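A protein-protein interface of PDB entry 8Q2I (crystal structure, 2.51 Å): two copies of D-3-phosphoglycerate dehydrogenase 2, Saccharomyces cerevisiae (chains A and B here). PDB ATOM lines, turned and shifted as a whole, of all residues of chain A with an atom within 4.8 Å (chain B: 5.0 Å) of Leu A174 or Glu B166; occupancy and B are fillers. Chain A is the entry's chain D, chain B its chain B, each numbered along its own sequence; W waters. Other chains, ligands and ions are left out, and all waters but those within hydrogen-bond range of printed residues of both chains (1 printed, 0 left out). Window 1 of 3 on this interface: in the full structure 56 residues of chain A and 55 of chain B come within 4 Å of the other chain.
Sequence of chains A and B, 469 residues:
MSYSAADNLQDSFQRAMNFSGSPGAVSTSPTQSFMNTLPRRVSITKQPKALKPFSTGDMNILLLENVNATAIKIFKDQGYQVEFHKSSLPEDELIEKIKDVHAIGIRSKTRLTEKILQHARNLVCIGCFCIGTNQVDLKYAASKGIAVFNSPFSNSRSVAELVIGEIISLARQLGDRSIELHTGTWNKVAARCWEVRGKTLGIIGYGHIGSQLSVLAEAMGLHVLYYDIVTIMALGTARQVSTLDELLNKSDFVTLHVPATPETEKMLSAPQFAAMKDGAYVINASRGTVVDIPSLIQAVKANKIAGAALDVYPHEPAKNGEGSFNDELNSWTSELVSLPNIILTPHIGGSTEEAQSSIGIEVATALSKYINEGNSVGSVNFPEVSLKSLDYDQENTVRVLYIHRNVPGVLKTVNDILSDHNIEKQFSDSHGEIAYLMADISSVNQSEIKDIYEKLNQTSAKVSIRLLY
1 position is printed for both chains. Of the 6 pairs that touch across the chains among the printed residues, none has its exchanged pair printed and touching as well.
Among the printed residues, pairs that only touch across the chains: Arg A172 with Leu B162 (3.7 Å), Leu A174 with Leu B162 (3.5 Å), Leu A174 with Glu B166 (3.97 Å), Leu A174 with Thr B345 (3.995 Å) and Ser A178 with Ile B343 (3.8 Å).
Water W1 bridges the side-chain hydroxyl of Ser A169 and the side-chain hydroxyl of Ser B169.
Printed residues of chain A that touch a printed residue of chain B: Arg A172, Leu A174 and Ser A178. Hydrophobic or aromatic side chains of chain A that line the printed part of chain B: Leu A174. Of the 15 printed residues of chain B, 5 touch a printed residue of chain A. Hydrophobic or aromatic side chains of chain B that line the printed part of chain A: Leu B162 and Ile B348.
Printed residues of chain B within 4 Å of Arg A172: Leu B162 (3.7 Å) and Ile B348 (3.2 Å). Of the printed residues of chain B, Leu A174 touches Leu B162 (3.5 Å), Glu B166 (3.97 Å) and Thr B345 (3.995 Å). Arg A177 touches none of the printed residues of chain B. Printed residues of chain B within 4 Å of Ser A178: Ile B343. Ile B164 touches none of the printed residues of chain A. Of the printed residues of chain A, Glu B166 touches Leu A174. Printed residues of chain A within 4 Å of Ile B343: Ser A178. Printed residues of chain A within 4 Å of Thr B345: Leu A174.
The backbone carbonyl oxygen (O) of Ser A169 sits at hydrogen-bond distance from the backbone NH (N) of Leu A174 (2.9 Å).
NH1 of Arg A172 lies within hydrogen-bond range of O of Ile B348, 3.2 Å away.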
ATOM      1  N   SER A 169       5.387  14.908 -24.953  1.00  0.00           N
ATOM      2  CA  SER A 169       5.368  15.471 -26.288  1.00  0.00           C
ATOM      3  C   SER A 169       4.383  16.651 -26.368  1.00  0.00           C
ATOM      4  O   SER A 169       4.654  17.668 -27.010  1.00  0.00           O
ATOM      5  CB  SER A 169       5.065  14.395 -27.286  1.00  0.00           C
ATOM      6  OG  SER A 169       4.889  14.988 -28.549  1.00  0.00           O
ATOM      7  N   ARG A 172       5.568  19.837 -24.497  1.00  0.00           N
ATOM      8  CA  ARG A 172       6.647  20.633 -25.112  1.00  0.00           C
ATOM      9  C   ARG A 172       6.355  20.858 -26.587  1.00  0.00           C
ATOM     10  O   ARG A 172       7.237  21.332 -27.283  1.00  0.00           O
ATOM     11  CB  ARG A 172       7.943  19.895 -24.784  1.00  0.00           C
ATOM     12  CG  ARG A 172       8.386  20.111 -23.345  1.00  0.00           C
ATOM     13  CD  ARG A 172       9.442  19.124 -22.913  1.00  0.00           C
ATOM     14  NE  ARG A 172      10.561  19.727 -22.208  1.00  0.00           N
ATOM     15  CZ  ARG A 172      11.578  20.330 -22.805  1.00  0.00           C
ATOM     16  NH1 ARG A 172      11.603  20.443 -24.120  1.00  0.00           N
ATOM     17  NH2 ARG A 172      12.564  20.830 -22.091  1.00  0.00           N
ATOM     18  N   GLN A 173       5.141  20.557 -27.017  1.00  0.00           N
ATOM     19  CA  GLN A 173       4.727  20.769 -28.397  1.00  0.00           C
ATOM     20  C   GLN A 173       5.722  20.168 -29.398  1.00  0.00           C
ATOM     21  O   GLN A 173       5.969  20.750 -30.459  1.00  0.00           O
ATOM     22  CB  GLN A 173       4.533  22.261 -28.662  1.00  0.00           C
ATOM     23  CG  GLN A 173       3.548  22.945 -27.716  1.00  0.00           C
ATOM     24  CD  GLN A 173       3.534  24.457 -27.815  1.00  0.00           C
ATOM     25  OE1 GLN A 173       4.094  25.064 -28.729  1.00  0.00           O
ATOM     26  NE2 GLN A 173       2.903  25.081 -26.835  1.00  0.00           N
ATOM     27  N   LEU A 174       6.250  18.973 -29.094  1.00  0.00           N
ATOM     28  CA  LEU A 174       7.264  18.349 -29.941  1.00  0.00           C
ATOM     29  C   LEU A 174       6.766  18.154 -31.361  1.00  0.00           C
ATOM     30  O   LEU A 174       7.499  18.390 -32.309  1.00  0.00           O
ATOM     31  CB  LEU A 174       7.657  16.974 -29.394  1.00  0.00           C
ATOM     32  CG  LEU A 174       8.589  16.937 -28.197  1.00  0.00           C
ATOM     33  CD1 LEU A 174       9.300  15.583 -28.158  1.00  0.00           C
ATOM     34  CD2 LEU A 174       9.604  18.072 -28.248  1.00  0.00           C
ATOM     35  N   GLY A 175       5.552  17.628 -31.491  1.00  0.00           N
ATOM     36  CA  GLY A 175       5.016  17.351 -32.807  1.00  0.00           C
ATOM     37  C   GLY A 175       4.996  18.594 -33.687  1.00  0.00           C
ATOM     38  O   GLY A 175       5.340  18.516 -34.863  1.00  0.00           O
ATOM     39  N   ASP A 176       4.597  19.722 -33.095  1.00  0.00           N
ATOM     40  CA  ASP A 176       4.465  20.979 -33.813  1.00  0.00           C
ATOM     41  C   ASP A 176       5.842  21.500 -34.238  1.00  0.00           C
ATOM     42  O   ASP A 176       6.013  22.009 -35.351  1.00  0.00           O
ATOM     43  CB  ASP A 176       3.742  22.015 -32.947  1.00  0.00           C
ATOM     44  CG  ASP A 176       2.217  21.955 -32.945  1.00  0.00           C
ATOM     45  OD1 ASP A 176       1.631  21.206 -33.773  1.00  0.00           O
ATOM     46  OD2 ASP A 176       1.609  22.692 -32.124  1.00  0.00           O
ATOM     47  N   ARG A 177       6.825  21.359 -33.334  1.00  0.00           N
ATOM     48  CA  ARG A 177       8.175  21.820 -33.581  1.00  0.00           C
ATOM     49  C   ARG A 177       8.753  21.095 -34.789  1.00  0.00           C
ATOM     50  O   ARG A 177       9.322  21.720 -35.689  1.00  0.00           O
ATOM     51  CB  ARG A 177       9.043  21.558 -32.351  1.00  0.00           C
ATOM     52  CG  ARG A 177       8.668  22.373 -31.119  1.00  0.00           C
ATOM     53  CD  ARG A 177       8.870  23.870 -31.315  1.00  0.00           C
ATOM     54  NE  ARG A 177       7.729  24.534 -31.920  1.00  0.00           N
ATOM     55  CZ  ARG A 177       6.598  24.827 -31.288  1.00  0.00           C
ATOM     56  NH1 ARG A 177       6.480  24.698 -29.976  1.00  0.00           N
ATOM     57  NH2 ARG A 177       5.572  25.229 -32.002  1.00  0.00           N
ATOM     58  N   SER A 178       8.597  19.765 -34.790  1.00  0.00           N
ATOM     59  CA  SER A 178       9.173  18.910 -35.815  1.00  0.00           C
ATOM     60  C   SER A 178       8.513  19.172 -37.172  1.00  0.00           C
ATOM     61  O   SER A 178       9.209  19.261 -38.178  1.00  0.00           O
ATOM     62  CB  SER A 178       9.106  17.457 -35.397  1.00  0.00           C
ATOM     63  OG  SER A 178       9.948  16.657 -36.219  1.00  0.00           O
ATOM     64  N   LEU B 162      13.004  15.884 -22.167  1.00  0.00           N
ATOM     65  CA  LEU B 162      12.874  15.894 -23.607  1.00  0.00           C
ATOM     66  C   LEU B 162      13.353  14.567 -24.192  1.00  0.00           C
ATOM     67  O   LEU B 162      12.753  14.024 -25.126  1.00  0.00           O
ATOM     68  CB  LEU B 162      13.721  17.018 -24.164  1.00  0.00           C
ATOM     69  CG  LEU B 162      13.733  17.080 -25.678  1.00  0.00           C
ATOM     70  CD1 LEU B 162      12.376  17.411 -26.175  1.00  0.00           C
ATOM     71  CD2 LEU B 162      14.714  18.109 -26.169  1.00  0.00           C
ATOM     72  N   VAL B 163      14.470  14.073 -23.657  1.00  0.00           N
ATOM     73  CA  VAL B 163      15.121  12.901 -24.200  1.00  0.00           C
ATOM     74  C   VAL B 163      14.258  11.672 -23.930  1.00  0.00           C
ATOM     75  O   VAL B 163      14.059  10.900 -24.866  1.00  0.00           O
ATOM     76  CB  VAL B 163      16.550  12.755 -23.642  1.00  0.00           C
ATOM     77  CG1 VAL B 163      17.114  11.364 -23.852  1.00  0.00           C
ATOM     78  CG2 VAL B 163      17.479  13.787 -24.268  1.00  0.00           C
ATOM     79  N   ILE B 164      13.742  11.510 -22.685  1.00  0.00           N
ATOM     80  CA  ILE B 164      12.846  10.408 -22.379  1.00  0.00           C
ATOM     81  C   ILE B 164      11.698  10.387 -23.390  1.00  0.00           C
ATOM     82  O   ILE B 164      11.279   9.330 -23.842  1.00  0.00           O
ATOM     83  CB  ILE B 164      12.301  10.450 -20.938  1.00  0.00           C
ATOM     84  CG1 ILE B 164      13.385  10.176 -19.893  1.00  0.00           C
ATOM     85  CG2 ILE B 164      11.130   9.469 -20.800  1.00  0.00           C
ATOM     86  CD1 ILE B 164      13.967   8.796 -19.957  1.00  0.00           C
ATOM     87  N   GLY B 165      11.191  11.553 -23.758  1.00  0.00           N
ATOM     88  CA  GLY B 165      10.061  11.633 -24.666  1.00  0.00           C
ATOM     89  C   GLY B 165      10.431  11.294 -26.108  1.00  0.00           C
ATOM     90  O   GLY B 165       9.592  10.780 -26.847  1.00  0.00           O
ATOM     91  N   GLU B 166      11.664  11.599 -26.499  1.00  0.00           N
ATOM     92  CA  GLU B 166      12.132  11.328 -27.843  1.00  0.00           C
ATOM     93  C   GLU B 166      12.520   9.854 -27.969  1.00  0.00           C
ATOM     94  O   GLU B 166      12.375   9.275 -29.026  1.00  0.00           O
ATOM     95  CB  GLU B 166      13.279  12.279 -28.175  1.00  0.00           C
ATOM     96  CG  GLU B 166      12.795  13.702 -28.343  1.00  0.00           C
ATOM     97  CD  GLU B 166      13.875  14.689 -28.772  1.00  0.00           C
ATOM     98  OE1 GLU B 166      15.003  14.577 -28.259  1.00  0.00           O
ATOM     99  OE2 GLU B 166      13.597  15.593 -29.619  1.00  0.00           O
ATOM    100  N   ILE B 167      13.027   9.248 -26.895  1.00  0.00           N
ATOM    101  CA  ILE B 167      13.272   7.819 -26.845  1.00  0.00           C
ATOM    102  C   ILE B 167      11.976   7.090 -27.199  1.00  0.00           C
ATOM    103  O   ILE B 167      11.927   6.281 -28.117  1.00  0.00           O
ATOM    104  CB  ILE B 167      13.837   7.405 -25.465  1.00  0.00           C
ATOM    105  CG1 ILE B 167      15.297   7.839 -25.296  1.00  0.00           C
ATOM    106  CG2 ILE B 167      13.704   5.907 -25.228  1.00  0.00           C
ATOM    107  CD1 ILE B 167      15.865   7.612 -23.900  1.00  0.00           C
ATOM    108  N   ILE B 168      10.911   7.413 -26.489  1.00  0.00           N
ATOM    109  CA  ILE B 168       9.638   6.749 -26.696  1.00  0.00           C
ATOM    110  C   ILE B 168       9.118   7.071 -28.092  1.00  0.00           C
ATOM    111  O   ILE B 168       8.656   6.183 -28.810  1.00  0.00           O
ATOM    112  CB  ILE B 168       8.630   7.139 -25.604  1.00  0.00           C
ATOM    113  CG1 ILE B 168       9.122   6.649 -24.239  1.00  0.00           C
ATOM    114  CG2 ILE B 168       7.256   6.622 -25.970  1.00  0.00           C
ATOM    115  CD1 ILE B 168       8.426   7.232 -23.043  1.00  0.00           C
ATOM    116  N   SER B 169       9.246   8.334 -28.478  1.00  0.00           N
ATOM    117  CA  SER B 169       8.687   8.775 -29.735  1.00  0.00           C
ATOM    118  C   SER B 169       9.361   8.090 -30.924  1.00  0.00           C
ATOM    119  O   SER B 169       8.717   7.704 -31.886  1.00  0.00           O
ATOM    120  CB  SER B 169       8.731  10.264 -29.817  1.00  0.00           C
ATOM    121  OG  SER B 169       8.332  10.672 -31.098  1.00  0.00           O
ATOM    122  N   LEU B 170      10.656   7.885 -30.821  1.00  0.00           N
ATOM    123  CA  LEU B 170      11.436   7.225 -31.859  1.00  0.00           C
ATOM    124  C   LEU B 170      11.148   5.718 -31.882  1.00  0.00           C
ATOM    125  O   LEU B 170      11.086   5.125 -32.959  1.00  0.00           O
ATOM    126  CB  LEU B 170      12.925   7.490 -31.602  1.00  0.00           C
ATOM    127  CG  LEU B 170      13.438   8.886 -31.978  1.00  0.00           C
ATOM    128  CD1 LEU B 170      14.925   8.970 -31.623  1.00  0.00           C
ATOM    129  CD2 LEU B 170      13.216   9.190 -33.464  1.00  0.00           C
ATOM    130  N   ALA B 171      11.035   5.124 -30.680  1.00  0.00           N
ATOM    131  CA  ALA B 171      10.748   3.712 -30.488  1.00  0.00           C
ATOM    132  C   ALA B 171       9.419   3.366 -31.150  1.00  0.00           C
ATOM    133  O   ALA B 171       9.235   2.242 -31.614  1.00  0.00           O
ATOM    134  CB  ALA B 171      10.734   3.346 -29.021  1.00  0.00           C
ATOM    135  N   ILE B 283      20.333  10.313 -30.445  1.00  0.00           N
ATOM    136  CA  ILE B 283      19.745  11.539 -29.927  1.00  0.00           C
ATOM    137  C   ILE B 283      20.843  12.525 -29.540  1.00  0.00           C
ATOM    138  O   ILE B 283      21.758  12.189 -28.779  1.00  0.00           O
ATOM    139  CB  ILE B 283      18.825  11.240 -28.737  1.00  0.00           C
ATOM    140  CG1 ILE B 283      17.753  10.221 -29.122  1.00  0.00           C
ATOM    141  CG2 ILE B 283      18.244  12.528 -28.183  1.00  0.00           C
ATOM    142  CD1 ILE B 283      17.036   9.615 -27.961  1.00  0.00           C
ATOM    143  N   ALA B 309      16.841  11.911 -33.239  1.00  0.00           N
ATOM    144  CA  ALA B 309      16.302  13.185 -32.797  1.00  0.00           C
ATOM    145  C   ALA B 309      17.429  14.191 -32.576  1.00  0.00           C
ATOM    146  O   ALA B 309      18.348  13.945 -31.804  1.00  0.00           O
ATOM    147  CB  ALA B 309      15.496  12.992 -31.543  1.00  0.00           C
ATOM    148  N   ILE B 343      13.116  13.128 -35.790  1.00  0.00           N
ATOM    149  CA  ILE B 343      12.593  14.234 -35.002  1.00  0.00           C
ATOM    150  C   ILE B 343      13.593  15.401 -34.991  1.00  0.00           C
ATOM    151  O   ILE B 343      14.732  15.264 -34.558  1.00  0.00           O
ATOM    152  CB  ILE B 343      12.314  13.762 -33.563  1.00  0.00           C
ATOM    153  CG1 ILE B 343      11.338  12.590 -33.523  1.00  0.00           C
ATOM    154  CG2 ILE B 343      11.896  14.936 -32.679  1.00  0.00           C
ATOM    155  CD1 ILE B 343      11.246  11.933 -32.172  1.00  0.00           C
ATOM    156  N   THR B 345      13.989  19.400 -33.607  1.00  0.00           N
ATOM    157  CA  THR B 345      13.505  20.451 -32.724  1.00  0.00           C
ATOM    158  C   THR B 345      14.448  21.658 -32.815  1.00  0.00           C
ATOM    159  O   THR B 345      15.640  21.504 -33.099  1.00  0.00           O
ATOM    160  CB  THR B 345      13.286  19.886 -31.312  1.00  0.00           C
ATOM    161  OG1 THR B 345      14.419  19.152 -30.853  1.00  0.00           O
ATOM    162  CG2 THR B 345      12.091  18.961 -31.246  1.00  0.00           C
ATOM    163  N   ILE B 348      15.141  23.513 -28.318  1.00  0.00           N
ATOM    164  CA  ILE B 348      14.129  23.688 -27.291  1.00  0.00           C
ATOM    165  C   ILE B 348      14.443  22.829 -26.060  1.00  0.00           C
ATOM    166  O   ILE B 348      13.624  22.728 -25.153  1.00  0.00           O
ATOM    167  CB  ILE B 348      12.715  23.453 -27.866  1.00  0.00           C
ATOM    168  CG1 ILE B 348      12.502  22.112 -28.568  1.00  0.00           C
ATOM    169  CG2 ILE B 348      12.361  24.575 -28.820  1.00  0.00           C
ATOM    170  CD1 ILE B 348      12.585  20.914 -27.675  1.00  0.00           C
HETATM  171  O   HOH W   1       6.133  13.090 -30.060  1.00  0.00           O
